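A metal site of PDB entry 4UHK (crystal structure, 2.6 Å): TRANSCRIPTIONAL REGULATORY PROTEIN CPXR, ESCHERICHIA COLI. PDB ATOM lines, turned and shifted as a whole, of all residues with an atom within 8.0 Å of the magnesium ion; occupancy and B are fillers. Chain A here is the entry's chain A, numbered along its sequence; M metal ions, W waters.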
ATOM      1  N   VAL A   7     -31.433  -9.016  14.559  1.00  0.00           N
ATOM      2  CA  VAL A   7     -30.637  -8.364  13.505  1.00  0.00           C
ATOM      3  C   VAL A   7     -29.601  -9.337  12.918  1.00  0.00           C
ATOM      4  O   VAL A   7     -28.524  -9.512  13.489  1.00  0.00           O
ATOM      5  CB  VAL A   7     -29.942  -7.043  13.999  1.00  0.00           C
ATOM      6  CG1 VAL A   7     -29.358  -6.251  12.832  1.00  0.00           C
ATOM      7  CG2 VAL A   7     -30.866  -6.177  14.865  1.00  0.00           C
ATOM      8  N   ASP A   8     -29.929  -9.933  11.755  1.00  0.00           N
ATOM      9  CA  ASP A   8     -29.084 -10.881  11.028  1.00  0.00           C
ATOM     10  C   ASP A   8     -29.461 -10.868   9.510  1.00  0.00           C
ATOM     11  O   ASP A   8     -30.620 -10.625   9.161  1.00  0.00           O
ATOM     12  CB  ASP A   8     -29.231 -12.306  11.631  1.00  0.00           C
ATOM     13  CG  ASP A   8     -28.030 -13.201  11.456  1.00  0.00           C
ATOM     14  OD1 ASP A   8     -27.660 -13.474  10.305  1.00  0.00           O
ATOM     15  OD2 ASP A   8     -27.451 -13.633  12.485  1.00  0.00           O
ATOM     16  N   ASP A   9     -28.481 -11.091   8.619  1.00  0.00           N
ATOM     17  CA  ASP A   9     -28.702 -11.085   7.174  1.00  0.00           C
ATOM     18  C   ASP A   9     -29.014 -12.506   6.667  1.00  0.00           C
ATOM     19  O   ASP A   9     -29.364 -12.690   5.509  1.00  0.00           O
ATOM     20  CB  ASP A   9     -27.507 -10.473   6.427  1.00  0.00           C
ATOM     21  CG  ASP A   9     -26.174 -11.170   6.630  1.00  0.00           C
ATOM     22  OD1 ASP A   9     -25.951 -11.760   7.729  1.00  0.00           O
ATOM     23  OD2 ASP A   9     -25.317 -11.042   5.733  1.00  0.00           O
ATOM     24  N   ASP A  10     -28.922 -13.497   7.551  1.00  0.00           N
ATOM     25  CA  ASP A  10     -29.251 -14.881   7.254  1.00  0.00           C
ATOM     26  C   ASP A  10     -30.757 -14.993   7.470  1.00  0.00           C
ATOM     27  O   ASP A  10     -31.224 -15.108   8.623  1.00  0.00           O
ATOM     28  CB  ASP A  10     -28.418 -15.823   8.161  1.00  0.00           C
ATOM     29  CG  ASP A  10     -28.552 -17.329   7.973  1.00  0.00           C
ATOM     30  OD1 ASP A  10     -29.582 -17.780   7.446  1.00  0.00           O
ATOM     31  OD2 ASP A  10     -27.674 -18.051   8.473  1.00  0.00           O
ATOM     32  N   LEU A  13     -32.049 -18.197   9.210  1.00  0.00           N
ATOM     33  CA  LEU A  13     -31.879 -18.176  10.665  1.00  0.00           C
ATOM     34  C   LEU A  13     -32.904 -17.250  11.319  1.00  0.00           C
ATOM     35  O   LEU A  13     -33.498 -17.624  12.336  1.00  0.00           O
ATOM     36  CB  LEU A  13     -30.444 -17.736  11.009  1.00  0.00           C
ATOM     37  CG  LEU A  13     -30.076 -17.721  12.471  1.00  0.00           C
ATOM     38  CD1 LEU A  13     -29.842 -19.128  12.995  1.00  0.00           C
ATOM     39  CD2 LEU A  13     -28.899 -16.824  12.685  1.00  0.00           C
ATOM     40  N   HIS A  32     -32.280  -6.916   8.651  1.00  0.00           N
ATOM     41  CA  HIS A  32     -31.356  -7.772   7.904  1.00  0.00           C
ATOM     42  C   HIS A  32     -29.991  -7.104   7.702  1.00  0.00           C
ATOM     43  O   HIS A  32     -29.119  -7.688   7.067  1.00  0.00           O
ATOM     44  CB  HIS A  32     -31.942  -8.225   6.573  1.00  0.00           C
ATOM     45  CG  HIS A  32     -33.203  -9.025   6.687  1.00  0.00           C
ATOM     46  ND1 HIS A  32     -34.398  -8.521   6.220  1.00  0.00           N
ATOM     47  CD2 HIS A  32     -33.429 -10.244   7.238  1.00  0.00           C
ATOM     48  CE1 HIS A  32     -35.319  -9.435   6.476  1.00  0.00           C
ATOM     49  NE2 HIS A  32     -34.782 -10.490   7.086  1.00  0.00           N
ATOM     50  N   PHD A  51     -26.091  -9.745  14.814  1.00  0.00           N
ATOM     51  CA  PHD A  51     -25.060 -10.441  14.028  1.00  0.00           C
ATOM     52  C   PHD A  51     -23.928  -9.424  13.835  1.00  0.00           C
ATOM     53  O   PHD A  51     -24.134  -8.237  14.067  1.00  0.00           O
ATOM     54  CB  PHD A  51     -25.662 -10.748  12.662  1.00  0.00           C
ATOM     55  CG  PHD A  51     -24.866 -11.720  11.783  1.00  0.00           C
ATOM     56  OD1 PHD A  51     -24.087 -12.727  12.359  1.00  0.00           O
ATOM     57  OD2 PHD A  51     -24.966 -11.659  10.562  1.00  0.00           O
ATOM     58  P   PHD A  51     -22.699 -13.198  11.776  1.00  0.00           P
ATOM     59  OP1 PHD A  51     -22.514 -14.630  12.198  1.00  0.00           O
ATOM     60  OP2 PHD A  51     -22.690 -13.134  10.266  1.00  0.00           O
ATOM     61  OP3 PHD A  51     -21.613 -12.300  12.336  1.00  0.00           O
ATOM     62  N   VAL A  52     -22.743  -9.878  13.401  1.00  0.00           N
ATOM     63  CA  VAL A  52     -21.630  -8.962  13.131  1.00  0.00           C
ATOM     64  C   VAL A  52     -21.500  -8.765  11.602  1.00  0.00           C
ATOM     65  O   VAL A  52     -21.590  -7.645  11.134  1.00  0.00           O
ATOM     66  CB  VAL A  52     -20.306  -9.401  13.768  1.00  0.00           C
ATOM     67  CG1 VAL A  52     -19.146  -8.566  13.237  1.00  0.00           C
ATOM     68  CG2 VAL A  52     -20.375  -9.302  15.297  1.00  0.00           C
ATOM     69  N   MET A  53     -21.299  -9.859  10.850  1.00  0.00           N
ATOM     70  CA  MET A  53     -21.060  -9.825   9.423  1.00  0.00           C
ATOM     71  C   MET A  53     -22.347  -9.660   8.658  1.00  0.00           C
ATOM     72  O   MET A  53     -23.075 -10.633   8.396  1.00  0.00           O
ATOM     73  CB  MET A  53     -20.274 -11.076   8.977  1.00  0.00           C
ATOM     74  CG  MET A  53     -18.959 -11.218   9.714  1.00  0.00           C
ATOM     75  SD  MET A  53     -18.103 -12.758   9.359  1.00  0.00           S
ATOM     76  CE  MET A  53     -19.179 -14.015  10.262  1.00  0.00           C
ATOM     77  N   MET A  54     -22.620  -8.402   8.293  1.00  0.00           N
ATOM     78  CA  MET A  54     -23.794  -8.012   7.524  1.00  0.00           C
ATOM     79  C   MET A  54     -23.430  -6.963   6.490  1.00  0.00           C
ATOM     80  O   MET A  54     -22.535  -6.168   6.741  1.00  0.00           O
ATOM     81  CB  MET A  54     -24.888  -7.440   8.446  1.00  0.00           C
ATOM     82  CG  MET A  54     -25.376  -8.392   9.515  1.00  0.00           C
ATOM     83  SD  MET A  54     -26.641  -7.587  10.486  1.00  0.00           S
ATOM     84  CE  MET A  54     -25.688  -6.231  11.277  1.00  0.00           C
ATOM     85  N   PRO A  55     -24.142  -6.856   5.340  1.00  0.00           N
ATOM     86  CA  PRO A  55     -23.857  -5.761   4.411  1.00  0.00           C
ATOM     87  C   PRO A  55     -24.458  -4.424   4.916  1.00  0.00           C
ATOM     88  O   PRO A  55     -25.174  -4.416   5.924  1.00  0.00           O
ATOM     89  CB  PRO A  55     -24.473  -6.217   3.097  1.00  0.00           C
ATOM     90  CG  PRO A  55     -25.393  -7.356   3.416  1.00  0.00           C
ATOM     91  CD  PRO A  55     -25.292  -7.683   4.882  1.00  0.00           C
ATOM     92  N   LEU A  77     -24.990 -12.361  18.614  1.00  0.00           N
ATOM     93  CA  LEU A  77     -25.256 -13.737  18.172  1.00  0.00           C
ATOM     94  C   LEU A  77     -24.548 -13.872  16.809  1.00  0.00           C
ATOM     95  O   LEU A  77     -25.069 -13.350  15.806  1.00  0.00           O
ATOM     96  CB  LEU A  77     -26.770 -13.967  18.127  1.00  0.00           C
ATOM     97  CG  LEU A  77     -27.234 -15.414  17.921  1.00  0.00           C
ATOM     98  CD1 LEU A  77     -26.649 -16.362  18.990  1.00  0.00           C
ATOM     99  CD2 LEU A  77     -28.776 -15.483  17.825  1.00  0.00           C
ATOM    100  N   THR A  78     -23.298 -14.429  16.798  1.00  0.00           N
ATOM    101  CA  THR A  78     -22.433 -14.364  15.633  1.00  0.00           C
ATOM    102  C   THR A  78     -21.409 -15.502  15.512  1.00  0.00           C
ATOM    103  O   THR A  78     -20.873 -15.950  16.521  1.00  0.00           O
ATOM    104  CB  THR A  78     -21.645 -13.000  15.689  1.00  0.00           C
ATOM    105  OG1 THR A  78     -20.578 -12.977  14.730  1.00  0.00           O
ATOM    106  CG2 THR A  78     -21.056 -12.712  17.052  1.00  0.00           C
ATOM    107  N   ALA A  79     -21.033 -15.815  14.233  1.00  0.00           N
ATOM    108  CA  ALA A  79     -20.038 -16.824  13.863  1.00  0.00           C
ATOM    109  C   ALA A  79     -18.635 -16.400  14.289  1.00  0.00           C
ATOM    110  O   ALA A  79     -17.736 -17.238  14.336  1.00  0.00           O
ATOM    111  CB  ALA A  79     -20.079 -17.071  12.369  1.00  0.00           C
ATOM    112  N   LYS A 100     -21.843 -18.653  17.198  1.00  0.00           N
ATOM    113  CA  LYS A 100     -22.517 -19.591  16.311  1.00  0.00           C
ATOM    114  C   LYS A 100     -21.543 -20.720  15.963  1.00  0.00           C
ATOM    115  O   LYS A 100     -20.376 -20.431  15.700  1.00  0.00           O
ATOM    116  CB  LYS A 100     -22.978 -18.911  15.022  1.00  0.00           C
ATOM    117  CG  LYS A 100     -24.220 -18.051  15.140  1.00  0.00           C
ATOM    118  CD  LYS A 100     -24.470 -17.422  13.790  1.00  0.00           C
ATOM    119  CE  LYS A 100     -25.452 -16.290  13.877  1.00  0.00           C
ATOM    120  NZ  LYS A 100     -25.490 -15.511  12.625  1.00  0.00           N
HETATM  121 MG    MG M   1     -24.107 -12.525   8.525  1.00  0.00          MG
HETATM  122  O   HOH W   1     -23.180 -12.665   6.090  1.00  0.00           O
HETATM  123  O   HOH W   2     -25.355 -14.210   9.100  1.00  0.00           O
HETATM  124  O   HOH W   3     -22.649 -14.711   7.541  1.00  0.00           O
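NZ of Lys 100 is in salt-bridge range of OP1 of PHD 51, at 3.1 Å. OP3 of PHD 51 is in hydrogen-bond range of the side-chain hydroxyl (OG1) of Thr 78, at 2.7 Å. OP1 of PHD 51 sits at hydrogen-bond distance from N of Ala 79 (2.8 Å). N of PHD 51 is in hydrogen-bond range of the backbone carbonyl oxygen (O) of Val 7, 2.8 Å away.
The magnesium ion is bound by OD1 of Asp 9 (2.1 Å), O of Met 53 (2.2 Å), water W2 (2.2 Å), OP2 of PHD 51 (2.3 Å) and OD2 of PHD 51 (2.4 Å). The magnesium ion has five donor atoms within binding distance. Slightly farther from the magnesium ion lies water W1 (2.6 Å). Slightly farther from the magnesium ion lies water W3 (2.8 Å).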
